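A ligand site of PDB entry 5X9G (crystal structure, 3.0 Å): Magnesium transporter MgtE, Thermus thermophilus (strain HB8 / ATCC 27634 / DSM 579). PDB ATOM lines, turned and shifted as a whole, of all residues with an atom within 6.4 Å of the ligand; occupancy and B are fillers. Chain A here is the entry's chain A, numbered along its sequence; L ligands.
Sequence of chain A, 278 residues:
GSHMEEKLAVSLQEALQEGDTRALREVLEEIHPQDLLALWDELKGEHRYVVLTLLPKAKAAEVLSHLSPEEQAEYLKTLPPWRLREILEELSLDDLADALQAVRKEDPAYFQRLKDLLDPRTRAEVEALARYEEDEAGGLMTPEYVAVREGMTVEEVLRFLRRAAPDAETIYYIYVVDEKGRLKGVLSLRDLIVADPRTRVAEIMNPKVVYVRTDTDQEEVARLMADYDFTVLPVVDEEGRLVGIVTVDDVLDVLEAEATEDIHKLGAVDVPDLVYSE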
ATOM      1  N   TYR A 172       0.973  -0.217  30.226  1.00  0.00           N
ATOM      2  CA  TYR A 172       2.306  -0.678  29.852  1.00  0.00           C
ATOM      3  C   TYR A 172       2.847   0.267  28.764  1.00  0.00           C
ATOM      4  O   TYR A 172       4.055   0.383  28.584  1.00  0.00           O
ATOM      5  CB  TYR A 172       2.314  -2.149  29.398  1.00  0.00           C
ATOM      6  CG  TYR A 172       1.774  -3.126  30.430  1.00  0.00           C
ATOM      7  CD1 TYR A 172       1.840  -2.857  31.775  1.00  0.00           C
ATOM      8  CD2 TYR A 172       1.244  -4.357  30.044  1.00  0.00           C
ATOM      9  CE1 TYR A 172       1.344  -3.744  32.718  1.00  0.00           C
ATOM     10  CE2 TYR A 172       0.759  -5.246  30.965  1.00  0.00           C
ATOM     11  CZ  TYR A 172       0.809  -4.931  32.306  1.00  0.00           C
ATOM     12  OH  TYR A 172       0.324  -5.801  33.257  1.00  0.00           O
ATOM     13  N   TYR A 173       1.964   0.949  28.057  1.00  0.00           N
ATOM     14  CA  TYR A 173       2.440   1.965  27.122  1.00  0.00           C
ATOM     15  C   TYR A 173       1.875   3.323  27.507  1.00  0.00           C
ATOM     16  O   TYR A 173       0.662   3.489  27.662  1.00  0.00           O
ATOM     17  CB  TYR A 173       2.069   1.595  25.694  1.00  0.00           C
ATOM     18  CG  TYR A 173       2.625   0.253  25.326  1.00  0.00           C
ATOM     19  CD1 TYR A 173       3.987   0.097  25.048  1.00  0.00           C
ATOM     20  CD2 TYR A 173       1.824  -0.895  25.349  1.00  0.00           C
ATOM     21  CE1 TYR A 173       4.516  -1.153  24.747  1.00  0.00           C
ATOM     22  CE2 TYR A 173       2.333  -2.134  25.050  1.00  0.00           C
ATOM     23  CZ  TYR A 173       3.679  -2.267  24.748  1.00  0.00           C
ATOM     24  OH  TYR A 173       4.198  -3.507  24.450  1.00  0.00           O
ATOM     25  N   TYR A 175       1.625   7.335  26.564  1.00  0.00           N
ATOM     26  CA  TYR A 175       1.720   8.155  25.369  1.00  0.00           C
ATOM     27  C   TYR A 175       1.983   9.619  25.674  1.00  0.00           C
ATOM     28  O   TYR A 175       1.625  10.127  26.739  1.00  0.00           O
ATOM     29  CB  TYR A 175       0.438   7.956  24.563  1.00  0.00           C
ATOM     30  CG  TYR A 175       0.334   6.535  24.031  1.00  0.00           C
ATOM     31  CD1 TYR A 175       0.879   6.206  22.798  1.00  0.00           C
ATOM     32  CD2 TYR A 175      -0.232   5.511  24.791  1.00  0.00           C
ATOM     33  CE1 TYR A 175       0.814   4.933  22.321  1.00  0.00           C
ATOM     34  CE2 TYR A 175      -0.289   4.224  24.320  1.00  0.00           C
ATOM     35  CZ  TYR A 175       0.240   3.941  23.082  1.00  0.00           C
ATOM     36  OH  TYR A 175       0.207   2.668  22.575  1.00  0.00           O
ATOM     37  N   VAL A 186       6.095   8.084  22.458  1.00  0.00           N
ATOM     38  CA  VAL A 186       5.638   6.905  23.187  1.00  0.00           C
ATOM     39  C   VAL A 186       6.736   6.259  24.039  1.00  0.00           C
ATOM     40  O   VAL A 186       7.905   6.239  23.668  1.00  0.00           O
ATOM     41  CB  VAL A 186       5.072   5.856  22.188  1.00  0.00           C
ATOM     42  CG1 VAL A 186       6.133   5.478  21.158  1.00  0.00           C
ATOM     43  CG2 VAL A 186       4.571   4.626  22.912  1.00  0.00           C
ATOM     44  N   LEU A 187       6.367   5.734  25.187  1.00  0.00           N
ATOM     45  CA  LEU A 187       7.332   5.010  25.983  1.00  0.00           C
ATOM     46  C   LEU A 187       6.617   3.881  26.728  1.00  0.00           C
ATOM     47  O   LEU A 187       5.421   3.948  26.963  1.00  0.00           O
ATOM     48  CB  LEU A 187       8.081   5.936  26.939  1.00  0.00           C
ATOM     49  CG  LEU A 187       7.414   6.671  28.099  1.00  0.00           C
ATOM     50  CD1 LEU A 187       8.397   6.913  29.231  1.00  0.00           C
ATOM     51  CD2 LEU A 187       6.873   8.003  27.608  1.00  0.00           C
ATOM     52  N   SER A 188       7.352   2.822  27.059  1.00  0.00           N
ATOM     53  CA  SER A 188       6.771   1.661  27.707  1.00  0.00           C
ATOM     54  C   SER A 188       6.945   1.756  29.197  1.00  0.00           C
ATOM     55  O   SER A 188       7.781   2.501  29.663  1.00  0.00           O
ATOM     56  CB  SER A 188       7.411   0.380  27.208  1.00  0.00           C
ATOM     57  OG  SER A 188       8.698   0.211  27.776  1.00  0.00           O
ATOM     58  N   LEU A 189       6.150   0.993  29.933  1.00  0.00           N
ATOM     59  CA  LEU A 189       6.303   0.929  31.388  1.00  0.00           C
ATOM     60  C   LEU A 189       7.667   0.395  31.835  1.00  0.00           C
ATOM     61  O   LEU A 189       8.194   0.770  32.889  1.00  0.00           O
ATOM     62  CB  LEU A 189       5.196   0.064  31.997  1.00  0.00           C
ATOM     63  CG  LEU A 189       5.230  -0.044  33.521  1.00  0.00           C
ATOM     64  CD1 LEU A 189       5.209   1.317  34.189  1.00  0.00           C
ATOM     65  CD2 LEU A 189       4.093  -0.879  34.009  1.00  0.00           C
ATOM     66  N   ARG A 190       8.236  -0.514  31.049  1.00  0.00           N
ATOM     67  CA  ARG A 190       9.548  -1.082  31.324  1.00  0.00           C
ATOM     68  C   ARG A 190      10.605   0.000  31.136  1.00  0.00           C
ATOM     69  O   ARG A 190      11.579   0.074  31.893  1.00  0.00           O
ATOM     70  CB  ARG A 190       9.778  -2.283  30.427  1.00  0.00           C
ATOM     71  CG  ARG A 190      11.078  -3.001  30.542  1.00  0.00           C
ATOM     72  CD  ARG A 190      10.877  -4.192  29.628  1.00  0.00           C
ATOM     73  NE  ARG A 190      11.803  -5.301  29.740  1.00  0.00           N
ATOM     74  CZ  ARG A 190      11.497  -6.479  29.224  1.00  0.00           C
ATOM     75  NH1 ARG A 190      10.334  -6.592  28.562  1.00  0.00           N
ATOM     76  NH2 ARG A 190      12.359  -7.489  29.370  1.00  0.00           N
ATOM     77  N   ASP A 191      10.400   0.874  30.140  1.00  0.00           N
ATOM     78  CA  ASP A 191      11.321   1.994  29.933  1.00  0.00           C
ATOM     79  C   ASP A 191      11.380   2.907  31.141  1.00  0.00           C
ATOM     80  O   ASP A 191      12.467   3.346  31.528  1.00  0.00           O
ATOM     81  CB  ASP A 191      10.926   2.823  28.705  1.00  0.00           C
ATOM     82  CG  ASP A 191      11.243   2.123  27.404  1.00  0.00           C
ATOM     83  OD1 ASP A 191      12.168   1.277  27.407  1.00  0.00           O
ATOM     84  OD2 ASP A 191      10.579   2.419  26.396  1.00  0.00           O
ATOM     85  N   ILE A 204      13.350   9.609  26.998  1.00  0.00           N
ATOM     86  CA  ILE A 204      13.210   8.149  26.978  1.00  0.00           C
ATOM     87  C   ILE A 204      12.260   7.736  25.889  1.00  0.00           C
ATOM     88  O   ILE A 204      12.304   6.634  25.351  1.00  0.00           O
ATOM     89  CB  ILE A 204      12.708   7.627  28.321  1.00  0.00           C
ATOM     90  CG1 ILE A 204      13.592   8.211  29.399  1.00  0.00           C
ATOM     91  CG2 ILE A 204      12.690   6.105  28.354  1.00  0.00           C
ATOM     92  CD1 ILE A 204      15.059   7.906  29.179  1.00  0.00           C
ATOM     93  N   MET A 205      11.382   8.670  25.590  1.00  0.00           N
ATOM     94  CA  MET A 205      10.336   8.419  24.644  1.00  0.00           C
ATOM     95  C   MET A 205      10.912   8.220  23.251  1.00  0.00           C
ATOM     96  O   MET A 205      11.913   8.830  22.852  1.00  0.00           O
ATOM     97  CB  MET A 205       9.346   9.581  24.646  1.00  0.00           C
ATOM     98  CG  MET A 205       9.864  10.827  23.984  1.00  0.00           C
ATOM     99  SD  MET A 205       8.641  12.126  24.052  1.00  0.00           S
ATOM    100  CE  MET A 205       8.878  12.908  22.464  1.00  0.00           C
ATOM    101  N   ASN A 206      10.198   7.404  22.496  1.00  0.00           N
ATOM    102  CA  ASN A 206      10.470   7.169  21.100  1.00  0.00           C
ATOM    103  C   ASN A 206       9.570   8.092  20.339  1.00  0.00           C
ATOM    104  O   ASN A 206       8.368   7.909  20.340  1.00  0.00           O
ATOM    105  CB  ASN A 206      10.228   5.696  20.762  1.00  0.00           C
ATOM    106  CG  ASN A 206      10.409   5.407  19.302  1.00  0.00           C
ATOM    107  OD1 ASN A 206      10.841   6.252  18.520  1.00  0.00           O
ATOM    108  ND2 ASN A 206      10.110   4.174  18.916  1.00  0.00           N
ATOM    109  N   LYS A 208       9.505   8.415  17.239  1.00  0.00           N
ATOM    110  CA  LYS A 208       9.094   7.730  16.025  1.00  0.00           C
ATOM    111  C   LYS A 208       7.875   6.844  16.310  1.00  0.00           C
ATOM    112  O   LYS A 208       7.970   5.622  16.391  1.00  0.00           O
ATOM    113  CB  LYS A 208      10.243   6.869  15.490  1.00  0.00           C
ATOM    114  CG  LYS A 208      11.508   7.618  15.087  1.00  0.00           C
ATOM    115  CD  LYS A 208      12.634   6.638  14.761  1.00  0.00           C
ATOM    116  CE  LYS A 208      12.098   5.414  13.997  1.00  0.00           C
ATOM    117  NZ  LYS A 208      13.088   4.309  13.910  1.00  0.00           N
ATOM    118  N   VAL A 209       6.713   7.496  16.465  1.00  0.00           N
ATOM    119  CA  VAL A 209       5.503   6.777  16.842  1.00  0.00           C
ATOM    120  C   VAL A 209       4.781   6.227  15.631  1.00  0.00           C
ATOM    121  O   VAL A 209       4.592   6.937  14.634  1.00  0.00           O
ATOM    122  CB  VAL A 209       4.513   7.675  17.603  1.00  0.00           C
ATOM    123  CG1 VAL A 209       3.323   6.872  18.024  1.00  0.00           C
ATOM    124  CG2 VAL A 209       5.164   8.232  18.832  1.00  0.00           C
ATOM    125  N   VAL A 210       4.390   4.956  15.687  1.00  0.00           N
ATOM    126  CA  VAL A 210       3.508   4.428  14.654  1.00  0.00           C
ATOM    127  C   VAL A 210       2.046   4.594  15.078  1.00  0.00           C
ATOM    128  O   VAL A 210       1.615   4.090  16.131  1.00  0.00           O
ATOM    129  CB  VAL A 210       3.818   2.958  14.339  1.00  0.00           C
ATOM    130  CG1 VAL A 210       5.143   2.857  13.624  1.00  0.00           C
ATOM    131  CG2 VAL A 210       3.790   2.135  15.582  1.00  0.00           C
ATOM    132  N   TYR A 211       1.295   5.304  14.233  1.00  0.00           N
ATOM    133  CA  TYR A 211      -0.075   5.654  14.567  1.00  0.00           C
ATOM    134  C   TYR A 211      -1.065   5.249  13.488  1.00  0.00           C
ATOM    135  O   TYR A 211      -0.704   4.874  12.391  1.00  0.00           O
ATOM    136  CB  TYR A 211      -0.209   7.149  14.824  1.00  0.00           C
ATOM    137  CG  TYR A 211       0.042   8.018  13.621  1.00  0.00           C
ATOM    138  CD1 TYR A 211      -1.002   8.334  12.747  1.00  0.00           C
ATOM    139  CD2 TYR A 211       1.301   8.560  13.350  1.00  0.00           C
ATOM    140  CE1 TYR A 211      -0.793   9.145  11.636  1.00  0.00           C
ATOM    141  CE2 TYR A 211       1.511   9.381  12.243  1.00  0.00           C
ATOM    142  CZ  TYR A 211       0.463   9.657  11.385  1.00  0.00           C
ATOM    143  OH  TYR A 211       0.631  10.459  10.276  1.00  0.00           O
ATOM    144  N   ASP A 229       5.101  -5.716  16.013  1.00  0.00           N
ATOM    145  CA  ASP A 229       4.972  -6.598  17.178  1.00  0.00           C
ATOM    146  C   ASP A 229       4.618  -5.786  18.424  1.00  0.00           C
ATOM    147  O   ASP A 229       5.207  -5.967  19.504  1.00  0.00           O
ATOM    148  CB  ASP A 229       6.270  -7.399  17.389  1.00  0.00           C
ATOM    149  CG  ASP A 229       6.648  -8.266  16.166  1.00  0.00           C
ATOM    150  OD1 ASP A 229       5.776  -8.888  15.487  1.00  0.00           O
ATOM    151  OD2 ASP A 229       7.873  -8.286  15.866  1.00  0.00           O
ATOM    152  N   PHE A 230       3.625  -4.913  18.262  1.00  0.00           N
ATOM    153  CA  PHE A 230       3.006  -4.138  19.347  1.00  0.00           C
ATOM    154  C   PHE A 230       1.705  -4.744  19.881  1.00  0.00           C
ATOM    155  O   PHE A 230       0.958  -5.355  19.131  1.00  0.00           O
ATOM    156  CB  PHE A 230       2.681  -2.743  18.858  1.00  0.00           C
ATOM    157  CG  PHE A 230       3.884  -1.908  18.594  1.00  0.00           C
ATOM    158  CD1 PHE A 230       4.933  -1.904  19.481  1.00  0.00           C
ATOM    159  CD2 PHE A 230       3.952  -1.122  17.458  1.00  0.00           C
ATOM    160  CE1 PHE A 230       6.049  -1.118  19.242  1.00  0.00           C
ATOM    161  CE2 PHE A 230       5.058  -0.335  17.219  1.00  0.00           C
ATOM    162  CZ  PHE A 230       6.107  -0.331  18.106  1.00  0.00           C
ATOM    163  N   VAL A 232      -0.560  -2.770  21.537  1.00  0.00           N
ATOM    164  CA  VAL A 232      -1.495  -1.646  21.571  1.00  0.00           C
ATOM    165  C   VAL A 232      -1.142  -0.672  20.466  1.00  0.00           C
ATOM    166  O   VAL A 232       0.005  -0.629  20.054  1.00  0.00           O
ATOM    167  CB  VAL A 232      -1.441  -0.931  22.915  1.00  0.00           C
ATOM    168  CG1 VAL A 232      -2.409   0.257  22.930  1.00  0.00           C
ATOM    169  CG2 VAL A 232      -1.726  -1.909  24.047  1.00  0.00           C
ATOM    170  N   LEU A 233      -2.113   0.052  19.930  1.00  0.00           N
ATOM    171  CA  LEU A 233      -1.766   1.014  18.906  1.00  0.00           C
ATOM    172  C   LEU A 233      -2.557   2.304  19.121  1.00  0.00           C
ATOM    173  O   LEU A 233      -3.726   2.264  19.424  1.00  0.00           O
ATOM    174  CB  LEU A 233      -2.016   0.435  17.523  1.00  0.00           C
ATOM    175  CG  LEU A 233      -0.891   0.610  16.511  1.00  0.00           C
ATOM    176  CD1 LEU A 233       0.415   0.226  17.123  1.00  0.00           C
ATOM    177  CD2 LEU A 233      -1.159  -0.266  15.320  1.00  0.00           C
ATOM    178  N   PRO A 234      -1.892   3.458  19.022  1.00  0.00           N
ATOM    179  CA  PRO A 234      -2.562   4.740  19.214  1.00  0.00           C
ATOM    180  C   PRO A 234      -3.356   5.250  17.999  1.00  0.00           C
ATOM    181  O   PRO A 234      -2.982   4.991  16.853  1.00  0.00           O
ATOM    182  CB  PRO A 234      -1.407   5.686  19.522  1.00  0.00           C
ATOM    183  CG  PRO A 234      -0.242   5.108  18.801  1.00  0.00           C
ATOM    184  CD  PRO A 234      -0.432   3.618  18.885  1.00  0.00           C
HETATM  185  P1  LIG L   1      12.025  -4.984  23.581  1.00  0.00           P
HETATM  186  O1  LIG L   1      11.508  -6.031  22.598  1.00  0.00           O
HETATM  187  O2  LIG L   1      13.494  -5.047  23.950  1.00  0.00           O
HETATM  188  O3  LIG L   1      11.568  -3.574  23.282  1.00  0.00           O
HETATM  189  P2  LIG L   1       9.702  -5.521  25.075  1.00  0.00           P
HETATM  190  O4  LIG L   1       9.292  -6.618  24.093  1.00  0.00           O
HETATM  191  O5  LIG L   1       9.292  -5.576  26.532  1.00  0.00           O
HETATM  192  O6  LIG L   1      11.309  -5.376  24.978  1.00  0.00           O
HETATM  193  P3  LIG L   1       8.445  -2.941  25.277  1.00  0.00           P
HETATM  194  O7  LIG L   1       7.140  -3.430  25.869  1.00  0.00           O
HETATM  195  O8  LIG L   1       9.427  -2.267  26.206  1.00  0.00           O
HETATM  196  O9  LIG L   1       9.226  -4.108  24.459  1.00  0.00           O
HETATM  197  O10 LIG L   1       8.115  -1.933  24.053  1.00  0.00           O
HETATM  198  C1  LIG L   1       8.975  -1.909  22.920  1.00  0.00           C
HETATM  199  C2  LIG L   1       9.383  -0.479  22.638  1.00  0.00           C
HETATM  200  O11 LIG L   1       8.715   0.014  21.472  1.00  0.00           O
HETATM  201  C3  LIG L   1       9.028   0.488  23.773  1.00  0.00           C
HETATM  202  O12 LIG L   1      10.162   0.738  24.607  1.00  0.00           O
HETATM  203  C4  LIG L   1       8.544   1.763  23.100  1.00  0.00           C
HETATM  204  O13 LIG L   1       9.529   2.795  23.199  1.00  0.00           O
HETATM  205  C5  LIG L   1       8.356   1.388  21.634  1.00  0.00           C
HETATM  206  N1  LIG L   1       6.928   1.481  21.293  1.00  0.00           N
HETATM  207  C6  LIG L   1       5.949   0.894  21.997  1.00  0.00           C
HETATM  208  N2  LIG L   1       4.739   1.151  21.440  1.00  0.00           N
HETATM  209  C7  LIG L   1       4.931   1.898  20.355  1.00  0.00           C
HETATM  210  C8  LIG L   1       4.063   2.502  19.313  1.00  0.00           C
HETATM  211  N3  LIG L   1       2.718   2.327  19.369  1.00  0.00           N
HETATM  212  N4  LIG L   1       4.659   3.231  18.347  1.00  0.00           N
HETATM  213  C9  LIG L   1       5.991   3.396  18.319  1.00  0.00           C
HETATM  214  N5  LIG L   1       6.844   2.870  19.229  1.00  0.00           N
HETATM  215  C10 LIG L   1       6.385   2.129  20.257  1.00  0.00           C
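An oxygen (O8) of the ligand sits at hydrogen-bond distance from the side-chain hydroxyl (OG) of Ser 188, 3.0 Å away. O12 of the ligand is in hydrogen-bond range of OD2 of Asp 191. N of Val 210 lies close to N4 of the ligand (3.2 Å). The side-chain hydroxyl of Tyr 173 lies within hydrogen-bond range of an oxygen (O7) of the ligand. NH1 of Arg 190 lies within salt-bridge range of O5 of the ligand (2.5 Å).
Merely in contact with the ligand: Val 186 (3.3 Å), Asn 206 (3.5 Å), Lys 208 (3.5 Å), Val 209 (3.7 Å), Phe 230 (3.3 Å), Leu 233 (3.8 Å) and Pro 234 (3.4 Å). Along chain A the residues within 4 Å of the ligand span positions 173 to 234.
The side-chain hydroxyl (OG) of Ser 188 lies within hydrogen-bond range of the backbone NH (N) of Asp 191, 3.0 Å away. The side-chain amide oxygen (OD1) of Asn 206 sits at hydrogen-bond distance from the backbone NH (N) of Lys 208 (2.8 Å). The side-chain hydroxyl (OG) of Ser 188 lies close to the backbone NH (N) of Arg 190, at 3.4 Å. O of Val 186 is in hydrogen-bond range of N of Asn 206 (2.8 Å).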
